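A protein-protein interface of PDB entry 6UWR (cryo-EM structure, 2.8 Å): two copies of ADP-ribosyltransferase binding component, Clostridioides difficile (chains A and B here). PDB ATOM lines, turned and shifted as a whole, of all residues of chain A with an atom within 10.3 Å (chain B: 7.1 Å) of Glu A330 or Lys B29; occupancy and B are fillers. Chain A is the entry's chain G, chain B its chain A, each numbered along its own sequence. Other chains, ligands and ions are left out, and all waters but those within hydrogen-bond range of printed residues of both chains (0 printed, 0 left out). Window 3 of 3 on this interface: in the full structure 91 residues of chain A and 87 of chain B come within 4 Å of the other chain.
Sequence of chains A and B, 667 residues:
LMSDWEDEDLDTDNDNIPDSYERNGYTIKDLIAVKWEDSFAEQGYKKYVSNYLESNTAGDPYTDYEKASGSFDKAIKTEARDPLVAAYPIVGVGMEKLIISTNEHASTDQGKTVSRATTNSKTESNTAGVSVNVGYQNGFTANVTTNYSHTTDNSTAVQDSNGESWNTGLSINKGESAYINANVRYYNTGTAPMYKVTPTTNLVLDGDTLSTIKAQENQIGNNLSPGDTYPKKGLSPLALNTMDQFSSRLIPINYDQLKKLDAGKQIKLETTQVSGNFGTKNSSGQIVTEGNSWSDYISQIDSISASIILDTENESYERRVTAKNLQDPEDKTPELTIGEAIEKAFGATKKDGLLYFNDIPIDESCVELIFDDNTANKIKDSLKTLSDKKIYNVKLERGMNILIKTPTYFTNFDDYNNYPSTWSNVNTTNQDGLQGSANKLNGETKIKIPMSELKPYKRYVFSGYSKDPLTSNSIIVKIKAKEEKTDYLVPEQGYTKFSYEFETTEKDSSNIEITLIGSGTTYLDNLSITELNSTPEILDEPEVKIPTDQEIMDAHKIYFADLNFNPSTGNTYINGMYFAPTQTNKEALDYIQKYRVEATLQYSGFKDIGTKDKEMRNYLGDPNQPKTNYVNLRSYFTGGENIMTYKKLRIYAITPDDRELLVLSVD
OE1 of Glu A330 lies within hydrogen-bond range of N of Asp B30, at 3.0 Å.
The guanidinium group (NH1) of Arg B81 is in salt-bridge range of the side-chain carboxylate (OD2) of Asp A328 (3.5 Å).
The side-chain hydroxyl (OH) of Tyr B45 lies close to the side-chain carboxylate (OE2) of Glu A330.
Among the printed residues, pairs that only touch across the chains: Pro A329 with Gly B44 (3.3 Å), Glu A330 with Lys B29 (3.4 Å), Glu A330 with Ile B28 (3.6 Å), Pro A329 with Tyr B45 (3.7 Å), Pro A329 with Gln B43 (3.8 Å) and Leu A53 with Leu B31 (3.9 Å).
Hydrophobic or aromatic side chains of chain B within 4 Å of the printed part of chain A: Leu B31 and Tyr B45.
Of the 18 printed residues of chain A, 4 touch a printed residue of chain B.
Among the printed residues, 9 pairs touch across the chains.
Among the printed residues, Asp or Glu carboxylates within 4 Å of a Lys or Arg side-chain nitrogen of the other chain: Asp A328 with Arg B81 (3.5 Å).
Of the printed residues of chain B, Leu A53 touches Leu B31.
Of the printed residues of chain B, Asp A328 touches Arg B81 (3.5 Å).
Glu A330 touches just these residues of chain B: Ile B28 (3.6 Å), Lys B29 (3.4 Å), Asp B30 (3.0 Å) and Tyr B45 (2.4 Å).
Ile B28 touches just one residue of chain A: Glu A330 (3.6 Å).
Lys B29 touches just one residue of chain A: Glu A330.
Printed residues of chain A within 4 Å of Tyr B45: Pro A329 and Glu A330.
Of the printed residues of chain A, Arg B81 touches Asp A328 (3.5 Å).
The nearest printed residue of chain A that does not touch Asp B30 is Tyr A52 (4.01 Å).
O of Phe B40 sits at hydrogen-bond distance from N of Tyr B45 (3.3 Å).
N of Leu A53 lies within hydrogen-bond range of OD1 of Asn A51 (3.0 Å).
OD1 of Asp A328 lies close to N of Glu A330 (3.3 Å).
NZ of Lys A332 sits at hydrogen-bond distance from O of Pro A329, 3.5 Å away.
No position is printed for both chains.
Of the 9 pairs that touch across the chains among the printed residues, none has its exchanged pair printed and touching as well.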
ATOM      1  N   THR A  12      26.093 -12.484  -5.926  1.00  0.00           N
ATOM      2  CA  THR A  12      24.851 -12.915  -6.549  1.00  0.00           C
ATOM      3  C   THR A  12      25.089 -13.805  -7.758  1.00  0.00           C
ATOM      4  O   THR A  12      24.284 -14.698  -8.031  1.00  0.00           O
ATOM      5  CB  THR A  12      24.019 -11.700  -6.947  1.00  0.00           C
ATOM      6  OG1 THR A  12      24.818 -10.524  -6.825  1.00  0.00           O
ATOM      7  CG2 THR A  12      22.837 -11.559  -6.026  1.00  0.00           C
ATOM      8  N   SER A  50      33.789  -5.854 -13.589  1.00  0.00           N
ATOM      9  CA  SER A  50      33.033  -6.879 -14.292  1.00  0.00           C
ATOM     10  C   SER A  50      31.572  -6.783 -13.884  1.00  0.00           C
ATOM     11  O   SER A  50      31.174  -5.900 -13.124  1.00  0.00           O
ATOM     12  CB  SER A  50      33.603  -8.265 -14.012  1.00  0.00           C
ATOM     13  OG  SER A  50      34.025  -8.380 -12.669  1.00  0.00           O
ATOM     14  N   ASN A  51      30.776  -7.706 -14.405  1.00  0.00           N
ATOM     15  CA  ASN A  51      29.343  -7.745 -14.162  1.00  0.00           C
ATOM     16  C   ASN A  51      29.084  -8.552 -12.898  1.00  0.00           C
ATOM     17  O   ASN A  51      29.453  -9.726 -12.819  1.00  0.00           O
ATOM     18  CB  ASN A  51      28.630  -8.359 -15.363  1.00  0.00           C
ATOM     19  CG  ASN A  51      27.140  -8.166 -15.323  1.00  0.00           C
ATOM     20  OD1 ASN A  51      26.571  -7.868 -14.284  1.00  0.00           O
ATOM     21  ND2 ASN A  51      26.496  -8.343 -16.458  1.00  0.00           N
ATOM     22  N   TYR A  52      28.464  -7.924 -11.907  1.00  0.00           N
ATOM     23  CA  TYR A  52      28.207  -8.603 -10.647  1.00  0.00           C
ATOM     24  C   TYR A  52      26.932  -9.426 -10.674  1.00  0.00           C
ATOM     25  O   TYR A  52      26.621 -10.084  -9.679  1.00  0.00           O
ATOM     26  CB  TYR A  52      28.151  -7.592  -9.502  1.00  0.00           C
ATOM     27  CG  TYR A  52      26.909  -6.743  -9.481  1.00  0.00           C
ATOM     28  CD1 TYR A  52      26.812  -5.609 -10.260  1.00  0.00           C
ATOM     29  CD2 TYR A  52      25.836  -7.074  -8.676  1.00  0.00           C
ATOM     30  CE1 TYR A  52      25.684  -4.837 -10.241  1.00  0.00           C
ATOM     31  CE2 TYR A  52      24.706  -6.312  -8.654  1.00  0.00           C
ATOM     32  CZ  TYR A  52      24.635  -5.192  -9.437  1.00  0.00           C
ATOM     33  OH  TYR A  52      23.502  -4.420  -9.413  1.00  0.00           O
ATOM     34  N   LEU A  53      26.191  -9.398 -11.776  1.00  0.00           N
ATOM     35  CA  LEU A  53      25.038 -10.259 -11.978  1.00  0.00           C
ATOM     36  C   LEU A  53      25.309 -11.329 -13.020  1.00  0.00           C
ATOM     37  O   LEU A  53      24.399 -12.070 -13.391  1.00  0.00           O
ATOM     38  CB  LEU A  53      23.825  -9.430 -12.389  1.00  0.00           C
ATOM     39  CG  LEU A  53      23.124  -8.598 -11.322  1.00  0.00           C
ATOM     40  CD1 LEU A  53      21.996  -7.837 -11.954  1.00  0.00           C
ATOM     41  CD2 LEU A  53      22.614  -9.484 -10.210  1.00  0.00           C
ATOM     42  N   GLU A  54      26.544 -11.422 -13.498  1.00  0.00           N
ATOM     43  CA  GLU A  54      26.933 -12.357 -14.544  1.00  0.00           C
ATOM     44  C   GLU A  54      28.195 -13.061 -14.090  1.00  0.00           C
ATOM     45  O   GLU A  54      29.158 -12.404 -13.687  1.00  0.00           O
ATOM     46  CB  GLU A  54      27.176 -11.627 -15.864  1.00  0.00           C
ATOM     47  CG  GLU A  54      26.948 -12.465 -17.092  1.00  0.00           C
ATOM     48  CD  GLU A  54      25.495 -12.827 -17.286  1.00  0.00           C
ATOM     49  OE1 GLU A  54      24.684 -11.918 -17.557  1.00  0.00           O
ATOM     50  OE2 GLU A  54      25.164 -14.025 -17.166  1.00  0.00           O
ATOM     51  N   LYS A 324      28.159  -2.649 -23.385  1.00  0.00           N
ATOM     52  CA  LYS A 324      26.967  -2.612 -22.556  1.00  0.00           C
ATOM     53  C   LYS A 324      25.742  -2.279 -23.397  1.00  0.00           C
ATOM     54  O   LYS A 324      25.827  -1.536 -24.377  1.00  0.00           O
ATOM     55  CB  LYS A 324      27.144  -1.585 -21.442  1.00  0.00           C
ATOM     56  CG  LYS A 324      25.892  -1.282 -20.663  1.00  0.00           C
ATOM     57  CD  LYS A 324      26.015   0.023 -19.924  1.00  0.00           C
ATOM     58  CE  LYS A 324      24.919   0.151 -18.903  1.00  0.00           C
ATOM     59  NZ  LYS A 324      24.631  -1.159 -18.279  1.00  0.00           N
ATOM     60  N   ASN A 325      24.604  -2.842 -23.014  1.00  0.00           N
ATOM     61  CA  ASN A 325      23.332  -2.588 -23.673  1.00  0.00           C
ATOM     62  C   ASN A 325      22.561  -1.548 -22.872  1.00  0.00           C
ATOM     63  O   ASN A 325      22.140  -1.819 -21.744  1.00  0.00           O
ATOM     64  CB  ASN A 325      22.529  -3.878 -23.795  1.00  0.00           C
ATOM     65  CG  ASN A 325      21.332  -3.733 -24.687  1.00  0.00           C
ATOM     66  OD1 ASN A 325      21.160  -2.718 -25.353  1.00  0.00           O
ATOM     67  ND2 ASN A 325      20.491  -4.754 -24.711  1.00  0.00           N
ATOM     68  N   LEU A 326      22.374  -0.363 -23.453  1.00  0.00           N
ATOM     69  CA  LEU A 326      21.698   0.707 -22.732  1.00  0.00           C
ATOM     70  C   LEU A 326      20.195   0.486 -22.644  1.00  0.00           C
ATOM     71  O   LEU A 326      19.572   0.904 -21.664  1.00  0.00           O
ATOM     72  CB  LEU A 326      21.986   2.051 -23.392  1.00  0.00           C
ATOM     73  CG  LEU A 326      23.437   2.517 -23.349  1.00  0.00           C
ATOM     74  CD1 LEU A 326      23.725   3.430 -24.521  1.00  0.00           C
ATOM     75  CD2 LEU A 326      23.728   3.217 -22.036  1.00  0.00           C
ATOM     76  N   GLN A 327      19.598  -0.164 -23.639  1.00  0.00           N
ATOM     77  CA  GLN A 327      18.169  -0.440 -23.611  1.00  0.00           C
ATOM     78  C   GLN A 327      17.790  -1.530 -22.617  1.00  0.00           C
ATOM     79  O   GLN A 327      16.622  -1.932 -22.583  1.00  0.00           O
ATOM     80  CB  GLN A 327      17.678  -0.831 -25.006  1.00  0.00           C
ATOM     81  CG  GLN A 327      18.013   0.184 -26.082  1.00  0.00           C
ATOM     82  CD  GLN A 327      17.742   1.606 -25.643  1.00  0.00           C
ATOM     83  OE1 GLN A 327      16.590   2.018 -25.514  1.00  0.00           O
ATOM     84  NE2 GLN A 327      18.804   2.365 -25.407  1.00  0.00           N
ATOM     85  N   ASP A 328      18.736  -2.021 -21.821  1.00  0.00           N
ATOM     86  CA  ASP A 328      18.449  -2.995 -20.782  1.00  0.00           C
ATOM     87  C   ASP A 328      18.863  -2.426 -19.438  1.00  0.00           C
ATOM     88  O   ASP A 328      20.059  -2.176 -19.226  1.00  0.00           O
ATOM     89  CB  ASP A 328      19.180  -4.304 -21.056  1.00  0.00           C
ATOM     90  CG  ASP A 328      18.638  -5.458 -20.239  1.00  0.00           C
ATOM     91  OD1 ASP A 328      17.663  -5.253 -19.488  1.00  0.00           O
ATOM     92  OD2 ASP A 328      19.188  -6.571 -20.346  1.00  0.00           O
ATOM     93  N   PRO A 329      17.935  -2.191 -18.508  1.00  0.00           N
ATOM     94  CA  PRO A 329      18.326  -1.673 -17.194  1.00  0.00           C
ATOM     95  C   PRO A 329      18.980  -2.705 -16.299  1.00  0.00           C
ATOM     96  O   PRO A 329      19.558  -2.330 -15.272  1.00  0.00           O
ATOM     97  CB  PRO A 329      16.997  -1.201 -16.603  1.00  0.00           C
ATOM     98  CG  PRO A 329      16.000  -2.065 -17.235  1.00  0.00           C
ATOM     99  CD  PRO A 329      16.476  -2.321 -18.630  1.00  0.00           C
ATOM    100  N   GLU A 330      18.907  -3.986 -16.650  1.00  0.00           N
ATOM    101  CA  GLU A 330      19.523  -5.048 -15.873  1.00  0.00           C
ATOM    102  C   GLU A 330      20.810  -5.552 -16.500  1.00  0.00           C
ATOM    103  O   GLU A 330      21.350  -6.566 -16.050  1.00  0.00           O
ATOM    104  CB  GLU A 330      18.542  -6.204 -15.689  1.00  0.00           C
ATOM    105  CG  GLU A 330      17.371  -5.871 -14.798  1.00  0.00           C
ATOM    106  CD  GLU A 330      17.805  -5.405 -13.430  1.00  0.00           C
ATOM    107  OE1 GLU A 330      18.666  -6.069 -12.820  1.00  0.00           O
ATOM    108  OE2 GLU A 330      17.288  -4.370 -12.962  1.00  0.00           O
ATOM    109  N   ASP A 331      21.303  -4.879 -17.532  1.00  0.00           N
ATOM    110  CA  ASP A 331      22.614  -5.178 -18.102  1.00  0.00           C
ATOM    111  C   ASP A 331      23.641  -4.379 -17.315  1.00  0.00           C
ATOM    112  O   ASP A 331      23.905  -3.216 -17.619  1.00  0.00           O
ATOM    113  CB  ASP A 331      22.652  -4.837 -19.584  1.00  0.00           C
ATOM    114  CG  ASP A 331      23.974  -5.192 -20.227  1.00  0.00           C
ATOM    115  OD1 ASP A 331      24.375  -6.366 -20.155  1.00  0.00           O
ATOM    116  OD2 ASP A 331      24.613  -4.298 -20.807  1.00  0.00           O
ATOM    117  N   LYS A 332      24.217  -5.003 -16.291  1.00  0.00           N
ATOM    118  CA  LYS A 332      25.152  -4.340 -15.396  1.00  0.00           C
ATOM    119  C   LYS A 332      26.591  -4.432 -15.873  1.00  0.00           C
ATOM    120  O   LYS A 332      27.509  -4.364 -15.055  1.00  0.00           O
ATOM    121  CB  LYS A 332      25.033  -4.922 -13.990  1.00  0.00           C
ATOM    122  CG  LYS A 332      23.623  -4.963 -13.467  1.00  0.00           C
ATOM    123  CD  LYS A 332      23.093  -3.576 -13.197  1.00  0.00           C
ATOM    124  CE  LYS A 332      21.729  -3.646 -12.556  1.00  0.00           C
ATOM    125  NZ  LYS A 332      21.198  -2.303 -12.236  1.00  0.00           N
ATOM    126  N   THR A 333      26.804  -4.590 -17.168  1.00  0.00           N
ATOM    127  CA  THR A 333      28.149  -4.720 -17.693  1.00  0.00           C
ATOM    128  C   THR A 333      28.845  -3.361 -17.629  1.00  0.00           C
ATOM    129  O   THR A 333      28.257  -2.348 -18.022  1.00  0.00           O
ATOM    130  CB  THR A 333      28.093  -5.228 -19.134  1.00  0.00           C
ATOM    131  OG1 THR A 333      27.996  -6.652 -19.123  1.00  0.00           O
ATOM    132  CG2 THR A 333      29.348  -4.871 -19.880  1.00  0.00           C
ATOM    133  N   PRO A 334      30.072  -3.294 -17.115  1.00  0.00           N
ATOM    134  CA  PRO A 334      30.744  -1.995 -16.998  1.00  0.00           C
ATOM    135  C   PRO A 334      30.837  -1.302 -18.346  1.00  0.00           C
ATOM    136  O   PRO A 334      30.995  -1.947 -19.383  1.00  0.00           O
ATOM    137  CB  PRO A 334      32.127  -2.357 -16.451  1.00  0.00           C
ATOM    138  CG  PRO A 334      31.938  -3.657 -15.795  1.00  0.00           C
ATOM    139  CD  PRO A 334      30.910  -4.382 -16.596  1.00  0.00           C
ATOM    140  N   ARG A 398      27.522  -2.463 -28.950  1.00  0.00           N
ATOM    141  CA  ARG A 398      27.460  -3.780 -29.562  1.00  0.00           C
ATOM    142  C   ARG A 398      27.334  -3.662 -31.071  1.00  0.00           C
ATOM    143  O   ARG A 398      26.583  -2.831 -31.584  1.00  0.00           O
ATOM    144  CB  ARG A 398      26.284  -4.567 -29.003  1.00  0.00           C
ATOM    145  CG  ARG A 398      26.321  -4.722 -27.512  1.00  0.00           C
ATOM    146  CD  ARG A 398      25.095  -5.422 -27.002  1.00  0.00           C
ATOM    147  NE  ARG A 398      25.267  -5.851 -25.624  1.00  0.00           N
ATOM    148  CZ  ARG A 398      24.494  -6.744 -25.025  1.00  0.00           C
ATOM    149  NH1 ARG A 398      23.494  -7.302 -25.689  1.00  0.00           N
ATOM    150  NH2 ARG A 398      24.720  -7.081 -23.767  1.00  0.00           N
ATOM    151  N   THR B  27       8.206  -8.382 -12.994  1.00  0.00           N
ATOM    152  CA  THR B  27       9.423  -8.074 -13.722  1.00  0.00           C
ATOM    153  C   THR B  27      10.588  -8.588 -12.895  1.00  0.00           C
ATOM    154  O   THR B  27      10.434  -8.943 -11.727  1.00  0.00           O
ATOM    155  CB  THR B  27       9.548  -6.578 -14.014  1.00  0.00           C
ATOM    156  OG1 THR B  27      10.385  -6.390 -15.158  1.00  0.00           O
ATOM    157  CG2 THR B  27      10.146  -5.847 -12.835  1.00  0.00           C
ATOM    158  N   ILE B  28      11.759  -8.643 -13.513  1.00  0.00           N
ATOM    159  CA  ILE B  28      12.945  -9.221 -12.897  1.00  0.00           C
ATOM    160  C   ILE B  28      13.969  -8.119 -12.713  1.00  0.00           C
ATOM    161  O   ILE B  28      14.384  -7.482 -13.688  1.00  0.00           O
ATOM    162  CB  ILE B  28      13.521 -10.363 -13.745  1.00  0.00           C
ATOM    163  CG1 ILE B  28      12.436 -11.395 -14.061  1.00  0.00           C
ATOM    164  CG2 ILE B  28      14.703 -10.991 -13.048  1.00  0.00           C
ATOM    165  CD1 ILE B  28      12.341 -12.519 -13.068  1.00  0.00           C
ATOM    166  N   LYS B  29      14.380  -7.887 -11.469  1.00  0.00           N
ATOM    167  CA  LYS B  29      15.502  -7.002 -11.196  1.00  0.00           C
ATOM    168  C   LYS B  29      16.416  -7.652 -10.172  1.00  0.00           C
ATOM    169  O   LYS B  29      15.949  -8.135  -9.137  1.00  0.00           O
ATOM    170  CB  LYS B  29      15.043  -5.626 -10.709  1.00  0.00           C
ATOM    171  CG  LYS B  29      13.966  -5.647  -9.669  1.00  0.00           C
ATOM    172  CD  LYS B  29      13.530  -4.237  -9.354  1.00  0.00           C
ATOM    173  CE  LYS B  29      13.150  -3.493 -10.612  1.00  0.00           C
ATOM    174  NZ  LYS B  29      12.904  -2.057 -10.335  1.00  0.00           N
ATOM    175  N   ASP B  30      17.714  -7.660 -10.477  1.00  0.00           N
ATOM    176  CA  ASP B  30      18.725  -8.352  -9.678  1.00  0.00           C
ATOM    177  C   ASP B  30      18.407  -9.836  -9.554  1.00  0.00           C
ATOM    178  O   ASP B  30      18.568 -10.441  -8.494  1.00  0.00           O
ATOM    179  CB  ASP B  30      18.893  -7.706  -8.306  1.00  0.00           C
ATOM    180  CG  ASP B  30      19.729  -6.446  -8.358  1.00  0.00           C
ATOM    181  OD1 ASP B  30      19.608  -5.692  -9.343  1.00  0.00           O
ATOM    182  OD2 ASP B  30      20.514  -6.210  -7.418  1.00  0.00           O
ATOM    183  N   LEU B  31      17.949 -10.421 -10.660  1.00  0.00           N
ATOM    184  CA  LEU B  31      17.734 -11.863 -10.784  1.00  0.00           C
ATOM    185  C   LEU B  31      16.662 -12.373  -9.831  1.00  0.00           C
ATOM    186  O   LEU B  31      16.642 -13.552  -9.482  1.00  0.00           O
ATOM    187  CB  LEU B  31      19.038 -12.636 -10.581  1.00  0.00           C
ATOM    188  CG  LEU B  31      20.160 -12.311 -11.563  1.00  0.00           C
ATOM    189  CD1 LEU B  31      21.340 -13.216 -11.324  1.00  0.00           C
ATOM    190  CD2 LEU B  31      19.672 -12.440 -12.984  1.00  0.00           C
ATOM    191  N   ILE B  32      15.753 -11.499  -9.412  1.00  0.00           N
ATOM    192  CA  ILE B  32      14.654 -11.862  -8.526  1.00  0.00           C
ATOM    193  C   ILE B  32      13.385 -11.227  -9.070  1.00  0.00           C
ATOM    194  O   ILE B  32      13.393 -10.057  -9.459  1.00  0.00           O
ATOM    195  CB  ILE B  32      14.908 -11.409  -7.077  1.00  0.00           C
ATOM    196  CG1 ILE B  32      16.138 -12.112  -6.511  1.00  0.00           C
ATOM    197  CG2 ILE B  32      13.711 -11.707  -6.211  1.00  0.00           C
ATOM    198  CD1 ILE B  32      16.396 -11.812  -5.060  1.00  0.00           C
ATOM    199  N   ALA B  33      12.302 -11.994  -9.107  1.00  0.00           N
ATOM    200  CA  ALA B  33      11.050 -11.496  -9.654  1.00  0.00           C
ATOM    201  C   ALA B  33      10.336 -10.616  -8.639  1.00  0.00           C
ATOM    202  O   ALA B  33      10.136 -11.012  -7.488  1.00  0.00           O
ATOM    203  CB  ALA B  33      10.155 -12.658 -10.067  1.00  0.00           C
ATOM    204  N   VAL B  34       9.948  -9.418  -9.066  1.00  0.00           N
ATOM    205  CA  VAL B  34       9.234  -8.480  -8.215  1.00  0.00           C
ATOM    206  C   VAL B  34       7.925  -8.111  -8.897  1.00  0.00           C
ATOM    207  O   VAL B  34       7.784  -8.206 -10.116  1.00  0.00           O
ATOM    208  CB  VAL B  34      10.065  -7.220  -7.909  1.00  0.00           C
ATOM    209  CG1 VAL B  34      11.387  -7.606  -7.299  1.00  0.00           C
ATOM    210  CG2 VAL B  34      10.286  -6.414  -9.159  1.00  0.00           C
ATOM    211  N   LYS B  35       6.956  -7.693  -8.088  1.00  0.00           N
ATOM    212  CA  LYS B  35       5.658  -7.319  -8.618  1.00  0.00           C
ATOM    213  C   LYS B  35       5.780  -6.105  -9.529  1.00  0.00           C
ATOM    214  O   LYS B  35       6.706  -5.303  -9.422  1.00  0.00           O
ATOM    215  CB  LYS B  35       4.680  -7.011  -7.489  1.00  0.00           C
ATOM    216  CG  LYS B  35       4.572  -8.093  -6.456  1.00  0.00           C
ATOM    217  CD  LYS B  35       3.767  -7.629  -5.265  1.00  0.00           C
ATOM    218  CE  LYS B  35       2.401  -7.141  -5.690  1.00  0.00           C
ATOM    219  NZ  LYS B  35       1.473  -7.022  -4.534  1.00  0.00           N
ATOM    220  N   GLU B  37       4.928  -2.498 -11.081  1.00  0.00           N
ATOM    221  CA  GLU B  37       4.431  -1.169 -10.775  1.00  0.00           C
ATOM    222  C   GLU B  37       4.699  -0.275 -11.973  1.00  0.00           C
ATOM    223  O   GLU B  37       5.802  -0.273 -12.521  1.00  0.00           O
ATOM    224  CB  GLU B  37       5.096  -0.589  -9.532  1.00  0.00           C
ATOM    225  CG  GLU B  37       5.086  -1.518  -8.342  1.00  0.00           C
ATOM    226  CD  GLU B  37       6.233  -1.261  -7.397  1.00  0.00           C
ATOM    227  OE1 GLU B  37       6.789  -0.145  -7.431  1.00  0.00           O
ATOM    228  OE2 GLU B  37       6.578  -2.173  -6.620  1.00  0.00           O
ATOM    229  N   PHE B  40       7.902   1.474 -13.193  1.00  0.00           N
ATOM    230  CA  PHE B  40       9.065   0.773 -13.721  1.00  0.00           C
ATOM    231  C   PHE B  40       9.237   0.943 -15.221  1.00  0.00           C
ATOM    232  O   PHE B  40      10.346   0.751 -15.724  1.00  0.00           O
ATOM    233  CB  PHE B  40       8.966  -0.721 -13.429  1.00  0.00           C
ATOM    234  CG  PHE B  40       9.092  -1.074 -11.985  1.00  0.00           C
ATOM    235  CD1 PHE B  40       9.529  -0.148 -11.066  1.00  0.00           C
ATOM    236  CD2 PHE B  40       8.780  -2.341 -11.550  1.00  0.00           C
ATOM    237  CE1 PHE B  40       9.647  -0.480  -9.745  1.00  0.00           C
ATOM    238  CE2 PHE B  40       8.895  -2.674 -10.233  1.00  0.00           C
ATOM    239  CZ  PHE B  40       9.331  -1.743  -9.329  1.00  0.00           C
ATOM    240  N   GLN B  43      11.706   3.518 -16.528  1.00  0.00           N
ATOM    241  CA  GLN B  43      13.061   3.083 -16.231  1.00  0.00           C
ATOM    242  C   GLN B  43      13.572   2.044 -17.218  1.00  0.00           C
ATOM    243  O   GLN B  43      14.773   1.758 -17.223  1.00  0.00           O
ATOM    244  CB  GLN B  43      13.127   2.538 -14.805  1.00  0.00           C
ATOM    245  CG  GLN B  43      12.727   3.558 -13.757  1.00  0.00           C
ATOM    246  CD  GLN B  43      12.422   2.932 -12.413  1.00  0.00           C
ATOM    247  OE1 GLN B  43      12.890   1.840 -12.103  1.00  0.00           O
ATOM    248  NE2 GLN B  43      11.630   3.623 -11.607  1.00  0.00           N
ATOM    249  N   GLY B  44      12.705   1.484 -18.045  1.00  0.00           N
ATOM    250  CA  GLY B  44      13.091   0.548 -19.070  1.00  0.00           C
ATOM    251  C   GLY B  44      12.733  -0.899 -18.824  1.00  0.00           C
ATOM    252  O   GLY B  44      13.346  -1.777 -19.439  1.00  0.00           O
ATOM    253  N   TYR B  45      11.769  -1.178 -17.959  1.00  0.00           N
ATOM    254  CA  TYR B  45      11.406  -2.543 -17.620  1.00  0.00           C
ATOM    255  C   TYR B  45      10.191  -2.989 -18.418  1.00  0.00           C
ATOM    256  O   TYR B  45       9.386  -2.180 -18.879  1.00  0.00           O
ATOM    257  CB  TYR B  45      11.136  -2.670 -16.124  1.00  0.00           C
ATOM    258  CG  TYR B  45      12.386  -2.621 -15.290  1.00  0.00           C
ATOM    259  CD1 TYR B  45      13.072  -3.776 -14.974  1.00  0.00           C
ATOM    260  CD2 TYR B  45      12.885  -1.421 -14.823  1.00  0.00           C
ATOM    261  CE1 TYR B  45      14.215  -3.738 -14.216  1.00  0.00           C
ATOM    262  CE2 TYR B  45      14.024  -1.373 -14.064  1.00  0.00           C
ATOM    263  CZ  TYR B  45      14.686  -2.533 -13.765  1.00  0.00           C
ATOM    264  OH  TYR B  45      15.829  -2.492 -13.006  1.00  0.00           O
ATOM    265  N   SER B  69      14.310 -13.590 -17.028  1.00  0.00           N
ATOM    266  CA  SER B  69      15.548 -13.129 -16.419  1.00  0.00           C
ATOM    267  C   SER B  69      16.657 -12.880 -17.429  1.00  0.00           C
ATOM    268  O   SER B  69      17.574 -12.110 -17.139  1.00  0.00           O
ATOM    269  CB  SER B  69      16.024 -14.149 -15.391  1.00  0.00           C
ATOM    270  OG  SER B  69      17.198 -13.712 -14.746  1.00  0.00           O
ATOM    271  N   ARG B  81      12.519 -12.814 -24.693  1.00  0.00           N
ATOM    272  CA  ARG B  81      12.659 -12.808 -23.249  1.00  0.00           C
ATOM    273  C   ARG B  81      11.325 -12.750 -22.535  1.00  0.00           C
ATOM    274  O   ARG B  81      11.288 -12.927 -21.316  1.00  0.00           O
ATOM    275  CB  ARG B  81      13.516 -11.628 -22.799  1.00  0.00           C
ATOM    276  CG  ARG B  81      14.986 -11.934 -22.740  1.00  0.00           C
ATOM    277  CD  ARG B  81      15.782 -10.672 -22.579  1.00  0.00           C
ATOM    278  NE  ARG B  81      15.425  -9.975 -21.353  1.00  0.00           N
ATOM    279  CZ  ARG B  81      16.310  -9.527 -20.474  1.00  0.00           C
ATOM    280  NH1 ARG B  81      17.604  -9.702 -20.698  1.00  0.00           N
ATOM    281  NH2 ARG B  81      15.905  -8.903 -19.377  1.00  0.00           N
